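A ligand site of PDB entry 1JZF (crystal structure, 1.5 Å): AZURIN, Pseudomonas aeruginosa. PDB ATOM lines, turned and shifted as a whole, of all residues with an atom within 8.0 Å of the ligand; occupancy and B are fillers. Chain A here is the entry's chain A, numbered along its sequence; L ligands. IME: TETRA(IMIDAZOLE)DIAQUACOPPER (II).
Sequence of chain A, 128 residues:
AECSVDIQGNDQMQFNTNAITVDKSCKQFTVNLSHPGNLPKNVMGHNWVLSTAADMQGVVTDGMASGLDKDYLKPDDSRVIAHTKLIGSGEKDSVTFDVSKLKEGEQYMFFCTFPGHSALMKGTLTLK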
ATOM      1  N   VAL A  22     -12.915  14.727  23.788  1.00  0.00           N
ATOM      2  CA  VAL A  22     -12.397  13.882  22.712  1.00  0.00           C
ATOM      3  C   VAL A  22     -11.180  14.593  22.115  1.00  0.00           C
ATOM      4  O   VAL A  22     -11.299  15.671  21.544  1.00  0.00           O
ATOM      5  CB  VAL A  22     -13.451  13.629  21.618  1.00  0.00           C
ATOM      6  CG1 VAL A  22     -12.842  12.840  20.471  1.00  0.00           C
ATOM      7  CG2 VAL A  22     -14.635  12.873  22.195  1.00  0.00           C
ATOM      8  N   ASP A  23     -10.012  13.981  22.303  1.00  0.00           N
ATOM      9  CA  ASP A  23      -8.767  14.539  21.783  1.00  0.00           C
ATOM     10  C   ASP A  23      -8.766  14.519  20.255  1.00  0.00           C
ATOM     11  O   ASP A  23      -9.122  13.513  19.646  1.00  0.00           O
ATOM     12  CB  ASP A  23      -7.576  13.738  22.328  1.00  0.00           C
ATOM     13  CG  ASP A  23      -6.241  14.470  22.160  1.00  0.00           C
ATOM     14  OD1 ASP A  23      -5.864  14.793  21.021  1.00  0.00           O
ATOM     15  OD2 ASP A  23      -5.567  14.703  23.187  1.00  0.00           O
ATOM     16  N   LYS A  24      -8.336  15.627  19.664  1.00  0.00           N
ATOM     17  CA  LYS A  24      -8.267  15.783  18.208  1.00  0.00           C
ATOM     18  C   LYS A  24      -7.374  14.760  17.521  1.00  0.00           C
ATOM     19  O   LYS A  24      -7.550  14.462  16.332  1.00  0.00           O
ATOM     20  CB  LYS A  24      -7.762  17.180  17.842  1.00  0.00           C
ATOM     21  CG  LYS A  24      -8.849  18.156  17.465  1.00  0.00           C
ATOM     22  CD  LYS A  24      -8.259  19.310  16.681  1.00  0.00           C
ATOM     23  CE  LYS A  24      -7.201  20.072  17.462  1.00  0.00           C
ATOM     24  NZ  LYS A  24      -6.779  21.310  16.759  1.00  0.00           N
ATOM     25  N   SER A  25      -6.387  14.252  18.249  1.00  0.00           N
ATOM     26  CA  SER A  25      -5.447  13.264  17.710  1.00  0.00           C
ATOM     27  C   SER A  25      -6.113  11.912  17.463  1.00  0.00           C
ATOM     28  O   SER A  25      -5.610  11.101  16.685  1.00  0.00           O
ATOM     29  CB  SER A  25      -4.264  13.088  18.664  1.00  0.00           C
ATOM     30  OG  SER A  25      -3.585  14.313  18.848  1.00  0.00           O
ATOM     31  N   CYS A  26      -7.237  11.676  18.138  1.00  0.00           N
ATOM     32  CA  CYS A  26      -7.973  10.422  17.993  1.00  0.00           C
ATOM     33  C   CYS A  26      -8.687  10.338  16.648  1.00  0.00           C
ATOM     34  O   CYS A  26      -9.274  11.317  16.189  1.00  0.00           O
ATOM     35  CB  CYS A  26      -9.011  10.276  19.112  1.00  0.00           C
ATOM     36  SG  CYS A  26      -8.335  10.228  20.803  1.00  0.00           S
ATOM     37  N   LYS A  27      -8.616   9.181  16.015  1.00  0.00           N
ATOM     38  CA  LYS A  27      -9.292   8.942  14.737  1.00  0.00           C
ATOM     39  C   LYS A  27     -10.674   8.396  15.063  1.00  0.00           C
ATOM     40  O   LYS A  27     -11.658   8.701  14.387  1.00  0.00           O
ATOM     41  CB  LYS A  27      -8.519   7.940  13.870  1.00  0.00           C
ATOM     42  CG  LYS A  27      -7.452   8.576  13.003  1.00  0.00           C
ATOM     43  CD  LYS A  27      -6.387   9.236  13.841  1.00  0.00           C
ATOM     44  CE  LYS A  27      -5.420  10.008  12.959  1.00  0.00           C
ATOM     45  NZ  LYS A  27      -4.486  10.836  13.767  1.00  0.00           N
ATOM     46  N   GLN A  28     -10.729   7.558  16.096  1.00  0.00           N
ATOM     47  CA  GLN A  28     -11.966   6.953  16.564  1.00  0.00           C
ATOM     48  C   GLN A  28     -12.049   7.146  18.077  1.00  0.00           C
ATOM     49  O   GLN A  28     -11.015   7.306  18.742  1.00  0.00           O
ATOM     50  CB  GLN A  28     -12.018   5.448  16.255  1.00  0.00           C
ATOM     51  CG  GLN A  28     -12.114   5.092  14.778  1.00  0.00           C
ATOM     52  CD  GLN A  28     -10.771   5.096  14.082  1.00  0.00           C
ATOM     53  OE1 GLN A  28      -9.761   4.695  14.642  1.00  0.00           O
ATOM     54  NE2 GLN A  28     -10.751   5.541  12.831  1.00  0.00           N
ATOM     55  N   PHE A  97     -17.009   5.446  17.220  1.00  0.00           N
ATOM     56  CA  PHE A  97     -17.387   6.316  16.118  1.00  0.00           C
ATOM     57  C   PHE A  97     -16.197   7.122  15.636  1.00  0.00           C
ATOM     58  O   PHE A  97     -15.236   7.329  16.380  1.00  0.00           O
ATOM     59  CB  PHE A  97     -18.541   7.246  16.510  1.00  0.00           C
ATOM     60  CG  PHE A  97     -18.234   8.172  17.665  1.00  0.00           C
ATOM     61  CD1 PHE A  97     -18.450   7.774  18.974  1.00  0.00           C
ATOM     62  CD2 PHE A  97     -17.727   9.449  17.424  1.00  0.00           C
ATOM     63  CE1 PHE A  97     -18.173   8.627  20.035  1.00  0.00           C
ATOM     64  CE2 PHE A  97     -17.445  10.311  18.487  1.00  0.00           C
ATOM     65  CZ  PHE A  97     -17.670   9.896  19.791  1.00  0.00           C
ATOM     66  N   ASP A  98     -16.249   7.559  14.377  1.00  0.00           N
ATOM     67  CA  ASP A  98     -15.180   8.354  13.789  1.00  0.00           C
ATOM     68  C   ASP A  98     -15.187   9.759  14.378  1.00  0.00           C
ATOM     69  O   ASP A  98     -16.228  10.429  14.402  1.00  0.00           O
ATOM     70  CB  ASP A  98     -15.331   8.434  12.264  1.00  0.00           C
ATOM     71  CG  ASP A  98     -15.183   7.074  11.595  1.00  0.00           C
ATOM     72  OD1 ASP A  98     -15.687   6.899  10.473  1.00  0.00           O
ATOM     73  OD2 ASP A  98     -14.556   6.165  12.180  1.00  0.00           O
ATOM     74  N   VAL A  99     -14.033  10.200  14.866  1.00  0.00           N
ATOM     75  CA  VAL A  99     -13.888  11.530  15.448  1.00  0.00           C
ATOM     76  C   VAL A  99     -14.149  12.632  14.415  1.00  0.00           C
ATOM     77  O   VAL A  99     -14.503  13.761  14.770  1.00  0.00           O
ATOM     78  CB  VAL A  99     -12.494  11.696  16.103  1.00  0.00           C
ATOM     79  CG1 VAL A  99     -12.275  13.117  16.570  1.00  0.00           C
ATOM     80  CG2 VAL A  99     -12.373  10.748  17.288  1.00  0.00           C
ATOM     81  N   SER A 100     -14.040  12.288  13.134  1.00  0.00           N
ATOM     82  CA  SER A 100     -14.281  13.232  12.052  1.00  0.00           C
ATOM     83  C   SER A 100     -15.755  13.601  11.953  1.00  0.00           C
ATOM     84  O   SER A 100     -16.117  14.497  11.200  1.00  0.00           O
ATOM     85  CB  SER A 100     -13.761  12.710  10.707  1.00  0.00           C
ATOM     86  OG  SER A 100     -14.377  11.496  10.303  1.00  0.00           O
ATOM     87  N   LYS A 101     -16.604  12.919  12.722  1.00  0.00           N
ATOM     88  CA  LYS A 101     -18.026  13.223  12.756  1.00  0.00           C
ATOM     89  C   LYS A 101     -18.266  14.393  13.710  1.00  0.00           C
ATOM     90  O   LYS A 101     -19.392  14.854  13.880  1.00  0.00           O
ATOM     91  CB  LYS A 101     -18.849  12.009  13.204  1.00  0.00           C
ATOM     92  CG  LYS A 101     -18.942  10.919  12.160  1.00  0.00           C
ATOM     93  CD  LYS A 101     -19.953   9.852  12.548  1.00  0.00           C
ATOM     94  CE  LYS A 101     -20.133   8.839  11.433  1.00  0.00           C
ATOM     95  NZ  LYS A 101     -18.861   8.144  11.101  1.00  0.00           N
ATOM     96  N   LEU A 102     -17.190  14.868  14.335  1.00  0.00           N
ATOM     97  CA  LEU A 102     -17.245  15.985  15.271  1.00  0.00           C
ATOM     98  C   LEU A 102     -16.382  17.126  14.765  1.00  0.00           C
ATOM     99  O   LEU A 102     -15.458  16.922  13.960  1.00  0.00           O
ATOM    100  CB  LEU A 102     -16.727  15.554  16.652  1.00  0.00           C
ATOM    101  CG  LEU A 102     -17.304  14.301  17.318  1.00  0.00           C
ATOM    102  CD1 LEU A 102     -16.567  14.049  18.620  1.00  0.00           C
ATOM    103  CD2 LEU A 102     -18.799  14.461  17.568  1.00  0.00           C
ATOM    104  N   LYS A 103     -16.659  18.331  15.239  1.00  0.00           N
ATOM    105  CA  LYS A 103     -15.894  19.513  14.839  1.00  0.00           C
ATOM    106  C   LYS A 103     -15.661  20.446  16.020  1.00  0.00           C
ATOM    107  O   LYS A 103     -16.420  20.449  16.984  1.00  0.00           O
ATOM    108  CB  LYS A 103     -16.589  20.264  13.701  1.00  0.00           C
ATOM    109  CG  LYS A 103     -17.857  21.007  14.098  1.00  0.00           C
ATOM    110  CD  LYS A 103     -18.450  21.745  12.903  1.00  0.00           C
ATOM    111  CE  LYS A 103     -19.664  22.572  13.316  1.00  0.00           C
ATOM    112  NZ  LYS A 103     -20.290  23.262  12.146  1.00  0.00           N
ATOM    113  N   GLU A 104     -14.579  21.222  15.937  1.00  0.00           N
ATOM    114  CA  GLU A 104     -14.231  22.174  16.976  1.00  0.00           C
ATOM    115  C   GLU A 104     -15.200  23.359  16.942  1.00  0.00           C
ATOM    116  O   GLU A 104     -15.657  23.750  15.866  1.00  0.00           O
ATOM    117  CB  GLU A 104     -12.828  22.708  16.774  1.00  0.00           C
ATOM    118  CG  GLU A 104     -11.732  21.665  16.855  1.00  0.00           C
ATOM    119  CD  GLU A 104     -10.352  22.283  16.952  1.00  0.00           C
ATOM    120  OE1 GLU A 104      -9.913  22.944  15.977  1.00  0.00           O
ATOM    121  OE2 GLU A 104      -9.693  22.123  18.001  1.00  0.00           O
ATOM    122  N   TYR A 108     -21.428  19.440  21.967  1.00  0.00           N
ATOM    123  CA  TYR A 108     -22.152  18.185  21.843  1.00  0.00           C
ATOM    124  C   TYR A 108     -22.665  17.770  23.206  1.00  0.00           C
ATOM    125  O   TYR A 108     -22.160  18.227  24.236  1.00  0.00           O
ATOM    126  CB  TYR A 108     -21.238  17.079  21.282  1.00  0.00           C
ATOM    127  CG  TYR A 108     -20.704  17.380  19.912  1.00  0.00           C
ATOM    128  CD1 TYR A 108     -21.472  17.168  18.779  1.00  0.00           C
ATOM    129  CD2 TYR A 108     -19.434  17.933  19.755  1.00  0.00           C
ATOM    130  CE1 TYR A 108     -21.004  17.506  17.516  1.00  0.00           C
ATOM    131  CE2 TYR A 108     -18.949  18.284  18.497  1.00  0.00           C
ATOM    132  CZ  TYR A 108     -19.741  18.067  17.381  1.00  0.00           C
ATOM    133  OH  TYR A 108     -19.292  18.454  16.141  1.00  0.00           O
ATOM    134  N   LEU A 127     -14.694  18.428  21.289  1.00  0.00           N
ATOM    135  CA  LEU A 127     -13.499  18.043  20.553  1.00  0.00           C
ATOM    136  C   LEU A 127     -12.426  19.085  20.837  1.00  0.00           C
ATOM    137  O   LEU A 127     -12.625  20.268  20.555  1.00  0.00           O
ATOM    138  CB  LEU A 127     -13.791  18.014  19.050  1.00  0.00           C
ATOM    139  CG  LEU A 127     -12.632  17.596  18.137  1.00  0.00           C
ATOM    140  CD1 LEU A 127     -12.272  16.150  18.407  1.00  0.00           C
ATOM    141  CD2 LEU A 127     -13.016  17.784  16.683  1.00  0.00           C
ATOM    142  N   LYS A 128     -11.330  18.674  21.443  1.00  0.00           N
ATOM    143  CA  LYS A 128     -10.244  19.608  21.721  1.00  0.00           C
ATOM    144  C   LYS A 128      -8.891  19.089  21.244  1.00  0.00           C
ATOM    145  O   LYS A 128      -8.654  17.867  21.322  1.00  0.00           O
ATOM    146  CB  LYS A 128     -10.181  19.964  23.217  1.00  0.00           C
ATOM    147  CG  LYS A 128     -10.881  21.275  23.548  1.00  0.00           C
ATOM    148  CD  LYS A 128     -12.061  21.062  24.473  1.00  0.00           C
ATOM    149  CE  LYS A 128     -11.822  21.720  25.822  1.00  0.00           C
ATOM    150  NZ  LYS A 128     -11.564  23.183  25.691  1.00  0.00           N
ATOM    151  OXT LYS A 128      -8.095  19.933  20.760  1.00  0.00           O
HETATM  152 CU   IME L   1      -8.972  14.799  12.220  1.00  0.00          CU
HETATM  153  O1  IME L   1      -9.438  13.693  14.767  1.00  0.00           O
HETATM  154  CG1 IME L   1     -12.882  16.940  11.713  1.00  0.00           C
HETATM  155  CDC IME L   1     -11.669  16.542  11.265  1.00  0.00           C
HETATM  156  NDB IME L   1     -12.981  16.487  13.007  1.00  0.00           N
HETATM  157  CEB IME L   1     -11.878  15.843  13.336  1.00  0.00           C
HETATM  158  NEC IME L   1     -11.064  15.868  12.301  1.00  0.00           N
HETATM  159  CG2 IME L   1     -10.218  11.150  10.588  1.00  0.00           C
HETATM  160  CDM IME L   1      -9.544  12.320  10.499  1.00  0.00           C
HETATM  161  NDL IME L   1     -10.815  11.138  11.831  1.00  0.00           N
HETATM  162  CEL IME L   1     -10.520  12.247  12.472  1.00  0.00           C
HETATM  163  NEM IME L   1      -9.741  12.991  11.692  1.00  0.00           N
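O1 of the ligand is in hydrogen-bond range of O of Lys 24.
NDB of the ligand sits close to O of Leu 102.
O of Cys 26 lies within hydrogen-bond range of O1 of the ligand, at 2.8 Å.
The side-chain carboxylate of Glu 104 lies within salt-bridge range of the side-chain amino group of Lys 24 (3.3 Å).
The backbone NH (N) of Lys 24 is in hydrogen-bond range of the chain-end carboxylate (O) of Lys 128 (2.8 Å).
The backbone NH of Val 99 is in hydrogen-bond range of the backbone carbonyl oxygen of Lys 27 (2.8 Å).
NZ of Lys 27 sits at hydrogen-bond distance from O of Ser 25, 3.1 Å away.
Merely in contact with the ligand: Lys 27 (3.6 Å), Val 99 (3.4 Å), Ser 100 (3.5 Å) and Leu 127 (3.9 Å).
Of the 18 residues printed, 7 come within 4 Å of the ligand.
Along chain A the residues within 4 Å of the ligand span positions 24 to 127.
The nearest printed residue that does not touch the ligand is Lys 103 (4.6 Å).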
